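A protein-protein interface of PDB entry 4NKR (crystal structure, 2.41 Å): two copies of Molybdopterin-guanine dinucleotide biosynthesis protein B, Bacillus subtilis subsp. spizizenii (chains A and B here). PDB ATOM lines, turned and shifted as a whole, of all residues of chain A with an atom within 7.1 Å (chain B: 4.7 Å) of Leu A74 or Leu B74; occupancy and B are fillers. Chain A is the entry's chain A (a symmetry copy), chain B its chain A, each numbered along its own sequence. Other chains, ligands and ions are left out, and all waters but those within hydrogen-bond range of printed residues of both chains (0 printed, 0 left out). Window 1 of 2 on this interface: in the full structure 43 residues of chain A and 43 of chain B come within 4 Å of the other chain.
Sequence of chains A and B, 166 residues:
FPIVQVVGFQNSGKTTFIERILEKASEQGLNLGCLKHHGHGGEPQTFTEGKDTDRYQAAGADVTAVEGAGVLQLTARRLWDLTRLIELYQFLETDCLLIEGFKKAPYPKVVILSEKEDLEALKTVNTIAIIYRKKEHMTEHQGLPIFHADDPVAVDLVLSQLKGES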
ATOM      1  N   CYS A  34      36.062  -0.119 -23.054  1.00  0.00           N
ATOM      2  CA  CYS A  34      36.244  -0.263 -24.463  1.00  0.00           C
ATOM      3  C   CYS A  34      35.918   1.038 -25.138  1.00  0.00           C
ATOM      4  O   CYS A  34      34.979   1.755 -24.753  1.00  0.00           O
ATOM      5  CB  CYS A  34      35.403  -1.413 -25.018  1.00  0.00           C
ATOM      6  SG  CYS A  34      35.982  -1.930 -26.664  1.00  0.00           S
ATOM      7  N   GLN A  57      19.069  16.962 -26.943  1.00  0.00           N
ATOM      8  CA  GLN A  57      20.269  17.200 -27.742  1.00  0.00           C
ATOM      9  C   GLN A  57      20.018  18.253 -28.820  1.00  0.00           C
ATOM     10  O   GLN A  57      20.856  19.103 -29.051  1.00  0.00           O
ATOM     11  CB  GLN A  57      20.780  15.890 -28.365  1.00  0.00           C
ATOM     12  CG  GLN A  57      22.233  15.931 -28.811  1.00  0.00           C
ATOM     13  CD  GLN A  57      23.232  16.147 -27.661  1.00  0.00           C
ATOM     14  OE1 GLN A  57      23.190  15.464 -26.631  1.00  0.00           O
ATOM     15  NE2 GLN A  57      24.144  17.091 -27.849  1.00  0.00           N
ATOM     16  N   ASP A  62      24.569  20.214 -24.694  1.00  0.00           N
ATOM     17  CA  ASP A  62      25.873  19.600 -25.060  1.00  0.00           C
ATOM     18  C   ASP A  62      26.143  18.250 -24.401  1.00  0.00           C
ATOM     19  O   ASP A  62      26.787  17.352 -25.027  1.00  0.00           O
ATOM     20  CB  ASP A  62      27.034  20.549 -24.590  1.00  0.00           C
ATOM     21  CG  ASP A  62      26.855  21.029 -23.075  1.00  0.00           C
ATOM     22  OD1 ASP A  62      25.717  20.877 -22.506  1.00  0.00           O
ATOM     23  OD2 ASP A  62      27.836  21.554 -22.464  1.00  0.00           O
ATOM     24  N   VAL A  63      25.756  18.166 -23.107  1.00  0.00           N
ATOM     25  CA  VAL A  63      25.927  16.974 -22.264  1.00  0.00           C
ATOM     26  C   VAL A  63      24.532  16.529 -21.813  1.00  0.00           C
ATOM     27  O   VAL A  63      23.890  17.216 -21.010  1.00  0.00           O
ATOM     28  CB  VAL A  63      26.818  17.331 -21.069  1.00  0.00           C
ATOM     29  CG1 VAL A  63      27.024  16.181 -20.126  1.00  0.00           C
ATOM     30  CG2 VAL A  63      28.167  17.795 -21.598  1.00  0.00           C
ATOM     31  N   THR A  64      24.054  15.413 -22.378  1.00  0.00           N
ATOM     32  CA  THR A  64      22.684  14.838 -22.108  1.00  0.00           C
ATOM     33  C   THR A  64      22.834  13.341 -21.759  1.00  0.00           C
ATOM     34  O   THR A  64      23.700  12.647 -22.294  1.00  0.00           O
ATOM     35  CB  THR A  64      21.723  14.848 -23.399  1.00  0.00           C
ATOM     36  OG1 THR A  64      22.374  14.219 -24.477  1.00  0.00           O
ATOM     37  CG2 THR A  64      21.327  16.233 -23.889  1.00  0.00           C
ATOM     38  N   ALA A  65      21.946  12.829 -20.918  1.00  0.00           N
ATOM     39  CA  ALA A  65      21.964  11.425 -20.516  1.00  0.00           C
ATOM     40  C   ALA A  65      20.626  10.866 -19.986  1.00  0.00           C
ATOM     41  O   ALA A  65      19.699  11.625 -19.566  1.00  0.00           O
ATOM     42  CB  ALA A  65      23.038  11.206 -19.484  1.00  0.00           C
ATOM     43  N   VAL A  66      20.531   9.532 -20.097  1.00  0.00           N
ATOM     44  CA  VAL A  66      19.478   8.724 -19.488  1.00  0.00           C
ATOM     45  C   VAL A  66      20.065   7.683 -18.588  1.00  0.00           C
ATOM     46  O   VAL A  66      21.030   7.005 -18.950  1.00  0.00           O
ATOM     47  CB  VAL A  66      18.623   7.969 -20.525  1.00  0.00           C
ATOM     48  CG1 VAL A  66      17.400   7.378 -19.826  1.00  0.00           C
ATOM     49  CG2 VAL A  66      18.110   8.929 -21.568  1.00  0.00           C
ATOM     50  N   LEU A  72      23.796   3.822 -17.613  1.00  0.00           N
ATOM     51  CA  LEU A  72      23.815   5.190 -18.036  1.00  0.00           C
ATOM     52  C   LEU A  72      24.073   5.222 -19.527  1.00  0.00           C
ATOM     53  O   LEU A  72      24.892   4.491 -20.003  1.00  0.00           O
ATOM     54  CB  LEU A  72      24.949   5.921 -17.330  1.00  0.00           C
ATOM     55  CG  LEU A  72      25.189   7.338 -17.812  1.00  0.00           C
ATOM     56  CD1 LEU A  72      24.033   8.230 -17.519  1.00  0.00           C
ATOM     57  CD2 LEU A  72      26.408   7.913 -17.131  1.00  0.00           C
ATOM     58  N   GLN A  73      23.300   6.009 -20.236  1.00  0.00           N
ATOM     59  CA  GLN A  73      23.538   6.295 -21.670  1.00  0.00           C
ATOM     60  C   GLN A  73      23.790   7.762 -21.828  1.00  0.00           C
ATOM     61  O   GLN A  73      22.930   8.579 -21.585  1.00  0.00           O
ATOM     62  CB  GLN A  73      22.327   5.892 -22.552  1.00  0.00           C
ATOM     63  CG  GLN A  73      21.819   4.496 -22.214  1.00  0.00           C
ATOM     64  CD  GLN A  73      22.185   3.422 -23.229  1.00  0.00           C
ATOM     65  OE1 GLN A  73      22.923   2.489 -22.919  1.00  0.00           O
ATOM     66  NE2 GLN A  73      21.579   3.500 -24.431  1.00  0.00           N
ATOM     67  N   LEU A  74      24.979   8.091 -22.213  1.00  0.00           N
ATOM     68  CA  LEU A  74      25.413   9.500 -22.164  1.00  0.00           C
ATOM     69  C   LEU A  74      25.896   9.934 -23.511  1.00  0.00           C
ATOM     70  O   LEU A  74      26.693   9.251 -24.141  1.00  0.00           O
ATOM     71  CB  LEU A  74      26.538   9.610 -21.095  1.00  0.00           C
ATOM     72  CG  LEU A  74      27.293  10.899 -20.769  1.00  0.00           C
ATOM     73  CD1 LEU A  74      28.471  11.030 -21.652  1.00  0.00           C
ATOM     74  CD2 LEU A  74      26.513  12.172 -20.800  1.00  0.00           C
ATOM     75  N   THR A  75      25.428  11.077 -23.953  1.00  0.00           N
ATOM     76  CA  THR A  75      26.047  11.757 -25.114  1.00  0.00           C
ATOM     77  C   THR A  75      26.654  13.125 -24.648  1.00  0.00           C
ATOM     78  O   THR A  75      25.976  13.943 -24.020  1.00  0.00           O
ATOM     79  CB  THR A  75      25.013  12.087 -26.167  1.00  0.00           C
ATOM     80  OG1 THR A  75      24.024  12.900 -25.527  1.00  0.00           O
ATOM     81  CG2 THR A  75      24.318  10.873 -26.663  1.00  0.00           C
ATOM     82  N   ALA A  76      27.903  13.379 -25.016  1.00  0.00           N
ATOM     83  CA  ALA A  76      28.634  14.560 -24.526  1.00  0.00           C
ATOM     84  C   ALA A  76      29.449  15.204 -25.636  1.00  0.00           C
ATOM     85  O   ALA A  76      30.427  14.654 -26.002  1.00  0.00           O
ATOM     86  CB  ALA A  76      29.562  14.173 -23.415  1.00  0.00           C
ATOM     87  N   ARG A  77      29.032  16.379 -26.114  1.00  0.00           N
ATOM     88  CA  ARG A  77      29.824  17.224 -27.066  1.00  0.00           C
ATOM     89  C   ARG A  77      30.917  18.113 -26.432  1.00  0.00           C
ATOM     90  O   ARG A  77      30.605  19.155 -25.916  1.00  0.00           O
ATOM     91  CB  ARG A  77      28.894  18.146 -27.854  1.00  0.00           C
ATOM     92  CG  ARG A  77      28.028  17.402 -28.824  1.00  0.00           C
ATOM     93  CD  ARG A  77      26.851  18.229 -29.370  1.00  0.00           C
ATOM     94  NE  ARG A  77      26.205  17.445 -30.430  1.00  0.00           N
ATOM     95  CZ  ARG A  77      26.732  17.281 -31.641  1.00  0.00           C
ATOM     96  NH1 ARG A  77      27.870  17.929 -31.971  1.00  0.00           N
ATOM     97  NH2 ARG A  77      26.131  16.479 -32.523  1.00  0.00           N
ATOM     98  N   TRP A  80      37.101  16.904 -27.337  1.00  0.00           N
ATOM     99  CA  TRP A  80      37.647  15.547 -26.974  1.00  0.00           C
ATOM    100  C   TRP A  80      38.914  15.206 -27.687  1.00  0.00           C
ATOM    101  O   TRP A  80      38.976  15.301 -28.889  1.00  0.00           O
ATOM    102  CB  TRP A  80      36.684  14.382 -27.288  1.00  0.00           C
ATOM    103  CG  TRP A  80      35.431  14.288 -26.390  1.00  0.00           C
ATOM    104  CD1 TRP A  80      34.127  14.454 -26.787  1.00  0.00           C
ATOM    105  CD2 TRP A  80      35.393  13.996 -25.003  1.00  0.00           C
ATOM    106  NE1 TRP A  80      33.301  14.297 -25.741  1.00  0.00           N
ATOM    107  CE2 TRP A  80      34.040  14.029 -24.615  1.00  0.00           C
ATOM    108  CE3 TRP A  80      36.366  13.719 -24.038  1.00  0.00           C
ATOM    109  CZ2 TRP A  80      33.623  13.827 -23.278  1.00  0.00           C
ATOM    110  CZ3 TRP A  80      35.939  13.483 -22.694  1.00  0.00           C
ATOM    111  CH2 TRP A  80      34.577  13.547 -22.351  1.00  0.00           C
ATOM    112  N   LEU A  88      38.403  10.075 -18.412  1.00  0.00           N
ATOM    113  CA  LEU A  88      37.007   9.700 -18.238  1.00  0.00           C
ATOM    114  C   LEU A  88      36.952   8.269 -17.814  1.00  0.00           C
ATOM    115  O   LEU A  88      36.256   7.956 -16.929  1.00  0.00           O
ATOM    116  CB  LEU A  88      36.193   9.938 -19.506  1.00  0.00           C
ATOM    117  CG  LEU A  88      34.686   9.555 -19.530  1.00  0.00           C
ATOM    118  CD1 LEU A  88      33.930  10.371 -18.543  1.00  0.00           C
ATOM    119  CD2 LEU A  88      34.037   9.717 -20.892  1.00  0.00           C
ATOM    120  N   TYR A  89      37.728   7.402 -18.421  1.00  0.00           N
ATOM    121  CA  TYR A  89      37.709   5.993 -18.054  1.00  0.00           C
ATOM    122  C   TYR A  89      38.255   5.727 -16.641  1.00  0.00           C
ATOM    123  O   TYR A  89      37.750   4.838 -15.943  1.00  0.00           O
ATOM    124  CB  TYR A  89      38.461   5.127 -19.069  1.00  0.00           C
ATOM    125  CG  TYR A  89      37.627   4.829 -20.280  1.00  0.00           C
ATOM    126  CD1 TYR A  89      37.505   5.755 -21.292  1.00  0.00           C
ATOM    127  CD2 TYR A  89      36.899   3.645 -20.391  1.00  0.00           C
ATOM    128  CE1 TYR A  89      36.698   5.513 -22.411  1.00  0.00           C
ATOM    129  CE2 TYR A  89      36.108   3.377 -21.528  1.00  0.00           C
ATOM    130  CZ  TYR A  89      35.986   4.320 -22.519  1.00  0.00           C
ATOM    131  OH  TYR A  89      35.183   4.115 -23.651  1.00  0.00           O
ATOM    132  N   LEU A  92      35.426   6.686 -14.195  1.00  0.00           N
ATOM    133  CA  LEU A  92      34.322   5.700 -14.059  1.00  0.00           C
ATOM    134  C   LEU A  92      34.887   4.409 -13.510  1.00  0.00           C
ATOM    135  O   LEU A  92      34.202   3.422 -13.457  1.00  0.00           O
ATOM    136  CB  LEU A  92      33.657   5.436 -15.409  1.00  0.00           C
ATOM    137  CG  LEU A  92      33.003   6.584 -16.164  1.00  0.00           C
ATOM    138  CD1 LEU A  92      32.647   6.190 -17.588  1.00  0.00           C
ATOM    139  CD2 LEU A  92      31.753   6.993 -15.430  1.00  0.00           C
ATOM    140  N   VAL B  63      31.698  -0.676 -19.437  1.00  0.00           N
ATOM    141  CA  VAL B  63      31.904   0.718 -19.856  1.00  0.00           C
ATOM    142  C   VAL B  63      32.414   0.689 -21.301  1.00  0.00           C
ATOM    143  O   VAL B  63      33.547   0.266 -21.552  1.00  0.00           O
ATOM    144  CB  VAL B  63      32.918   1.377 -18.914  1.00  0.00           C
ATOM    145  CG1 VAL B  63      33.223   2.800 -19.284  1.00  0.00           C
ATOM    146  CG2 VAL B  63      32.358   1.335 -17.500  1.00  0.00           C
ATOM    147  N   THR B  64      31.549   1.089 -22.242  1.00  0.00           N
ATOM    148  CA  THR B  64      31.837   1.087 -23.724  1.00  0.00           C
ATOM    149  C   THR B  64      31.485   2.476 -24.300  1.00  0.00           C
ATOM    150  O   THR B  64      30.537   3.125 -23.858  1.00  0.00           O
ATOM    151  CB  THR B  64      30.909   0.068 -24.553  1.00  0.00           C
ATOM    152  OG1 THR B  64      29.555   0.321 -24.264  1.00  0.00           O
ATOM    153  CG2 THR B  64      31.143  -1.404 -24.245  1.00  0.00           C
ATOM    154  N   ALA B  65      32.202   2.896 -25.334  1.00  0.00           N
ATOM    155  CA  ALA B  65      31.963   4.183 -25.984  1.00  0.00           C
ATOM    156  C   ALA B  65      32.482   4.304 -27.432  1.00  0.00           C
ATOM    157  O   ALA B  65      33.368   3.524 -27.897  1.00  0.00           O
ATOM    158  CB  ALA B  65      32.552   5.289 -25.150  1.00  0.00           C
ATOM    159  N   LEU B  72      30.940  12.217 -27.978  1.00  0.00           N
ATOM    160  CA  LEU B  72      31.138  10.965 -27.313  1.00  0.00           C
ATOM    161  C   LEU B  72      29.781  10.346 -27.054  1.00  0.00           C
ATOM    162  O   LEU B  72      28.879  11.034 -26.671  1.00  0.00           O
ATOM    163  CB  LEU B  72      31.825  11.206 -25.975  1.00  0.00           C
ATOM    164  CG  LEU B  72      31.943   9.981 -25.091  1.00  0.00           C
ATOM    165  CD1 LEU B  72      32.824   8.941 -25.694  1.00  0.00           C
ATOM    166  CD2 LEU B  72      32.526  10.367 -23.753  1.00  0.00           C
ATOM    167  N   GLN B  73      29.651   9.077 -27.358  1.00  0.00           N
ATOM    168  CA  GLN B  73      28.456   8.280 -26.999  1.00  0.00           C
ATOM    169  C   GLN B  73      28.878   7.173 -26.083  1.00  0.00           C
ATOM    170  O   GLN B  73      29.618   6.293 -26.460  1.00  0.00           O
ATOM    171  CB  GLN B  73      27.766   7.668 -28.247  1.00  0.00           C
ATOM    172  CG  GLN B  73      27.587   8.698 -29.357  1.00  0.00           C
ATOM    173  CD  GLN B  73      26.163   9.207 -29.529  1.00  0.00           C
ATOM    174  OE1 GLN B  73      25.887  10.386 -29.320  1.00  0.00           O
ATOM    175  NE2 GLN B  73      25.265   8.326 -30.014  1.00  0.00           N
ATOM    176  N   LEU B  74      28.423   7.236 -24.876  1.00  0.00           N
ATOM    177  CA  LEU B  74      28.965   6.347 -23.830  1.00  0.00           C
ATOM    178  C   LEU B  74      27.855   5.579 -23.185  1.00  0.00           C
ATOM    179  O   LEU B  74      26.843   6.147 -22.797  1.00  0.00           O
ATOM    180  CB  LEU B  74      29.713   7.238 -22.797  1.00  0.00           C
ATOM    181  CG  LEU B  74      30.381   6.709 -21.527  1.00  0.00           C
ATOM    182  CD1 LEU B  74      29.405   6.686 -20.417  1.00  0.00           C
ATOM    183  CD2 LEU B  74      31.055   5.379 -21.616  1.00  0.00           C
ATOM    184  N   THR B  75      28.045   4.288 -23.055  1.00  0.00           N
ATOM    185  CA  THR B  75      27.174   3.474 -22.177  1.00  0.00           C
ATOM    186  C   THR B  75      28.030   2.887 -21.002  1.00  0.00           C
ATOM    187  O   THR B  75      29.072   2.263 -21.221  1.00  0.00           O
ATOM    188  CB  THR B  75      26.605   2.288 -22.923  1.00  0.00           C
ATOM    189  OG1 THR B  75      27.722   1.543 -23.418  1.00  0.00           O
ATOM    190  CG2 THR B  75      25.806   2.704 -24.101  1.00  0.00           C
ATOM    191  N   ALA B  76      27.545   3.040 -19.777  1.00  0.00           N
ATOM    192  CA  ALA B  76      28.317   2.662 -18.581  1.00  0.00           C
ATOM    193  C   ALA B  76      27.435   1.982 -17.547  1.00  0.00           C
ATOM    194  O   ALA B  76      26.672   2.646 -16.939  1.00  0.00           O
ATOM    195  CB  ALA B  76      28.937   3.875 -17.956  1.00  0.00           C
ATOM    196  N   LEU B  92      32.673  16.488 -16.406  1.00  0.00           N
ATOM    197  CA  LEU B  92      32.615  16.853 -17.846  1.00  0.00           C
ATOM    198  C   LEU B  92      32.437  18.351 -17.961  1.00  0.00           C
ATOM    199  O   LEU B  92      32.216  18.854 -19.031  1.00  0.00           O
ATOM    200  CB  LEU B  92      31.456  16.143 -18.543  1.00  0.00           C
ATOM    201  CG  LEU B  92      31.412  14.622 -18.571  1.00  0.00           C
ATOM    202  CD1 LEU B  92      30.066  14.108 -19.056  1.00  0.00           C
ATOM    203  CD2 LEU B  92      32.498  14.126 -19.489  1.00  0.00           C
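Val A63 touches Leu B92, and with the chains exchanged Leu A92 touches Val B63. Leu A72 touches Leu B74, and with the chains exchanged Leu A74 touches Leu B72. Gln A73 touches Thr B75, and with the chains exchanged Thr A75 touches Gln B73. Leu B74 touches its own counterpart, Leu A74. 9 positions are printed for both chains. Of the 21 pairs that touch across the chains among the printed residues, 13 have their exchanged pair printed and touching as well.
Among the printed residues, pairs that only touch across the chains: Cys A34 with Thr B64, Val A63 with Leu B92, Leu A72 with Leu B74, Leu A72 with Thr B75, Gln A73 with Leu B74, Gln A73 with Thr B75, Leu A74 with Leu B72, Leu A74 with Gln B73, Thr A75 with Leu B72, Thr A75 with Gln B73, Trp A80 with Leu B72, Trp A80 with Leu B92, Leu A88 with Leu B72, Tyr A89 with Val B63, Tyr A89 with Ala B65 and Leu A92 with Val B63.
Of the 17 printed residues of chain A, 11 touch a printed residue of chain B. Hydrophobic or aromatic side chains of chain A within 4 Å of the printed part of chain B: Val A63, Leu A72, Leu A74, Trp A80, Leu A88, Tyr A89 and Leu A92. Hydrophobic or aromatic side chains of chain B within 4 Å of the printed part of chain A: Val B63, Ala B65, Leu B72, Leu B74 and Leu B92. Among the printed residues, no Asp or Glu carboxylate lies within 4 Å of a Lys or Arg side-chain nitrogen of the other chain.
The backbone NH of Thr B75 lies within hydrogen-bond range of the backbone carbonyl oxygen of Thr B64. The side-chain hydroxyl of Tyr A89 sits at hydrogen-bond distance from the backbone carbonyl oxygen of Cys A34, 2.6 Å away. The side-chain amide oxygen of Gln A57 is in hydrogen-bond range of the side-chain hydroxyl of Thr A75, 2.9 Å away. The backbone NH of Thr A75 is in hydrogen-bond range of the backbone carbonyl oxygen of Thr A64, at 2.9 Å. N of Gln A73 sits at hydrogen-bond distance from O of Val A66, at 2.8 Å. The indole nitrogen (NE1) of Trp A80 sits at hydrogen-bond distance from the backbone carbonyl oxygen (O) of Ala A76, at 2.9 Å.
O of Val B63 sits at hydrogen-bond distance from N of Cys A34 (3.0 Å). The backbone NH (N) of Ala B65 lies within hydrogen-bond range of the backbone carbonyl oxygen (O) of Cys A34, at 3.1 Å. The backbone carbonyl oxygen (O) of Leu B72 lies within hydrogen-bond range of the backbone NH (N) of Ala A76 (3.0 Å). N of Leu A74 lies within hydrogen-bond range of O of Leu B74. The backbone carbonyl oxygen of Leu A72 sits at hydrogen-bond distance from the backbone NH of Ala B76, at 3.0 Å.
Of the printed residues of chain B, Cys A34 touches Val B63, Thr B64 and Ala B65. Of the printed residues of chain B, Gln A73 touches Leu B74 (3.5 Å) and Thr B75 (3.1 Å). Of chain B, only Leu B72, Gln B73 and Leu B74 come within 4 Å of Leu A74. Of the printed residues of chain B, Thr A75 touches Leu B72 (3.3 Å) and Gln B73 (3.1 Å). Leu B74 touches three residues of chain A.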
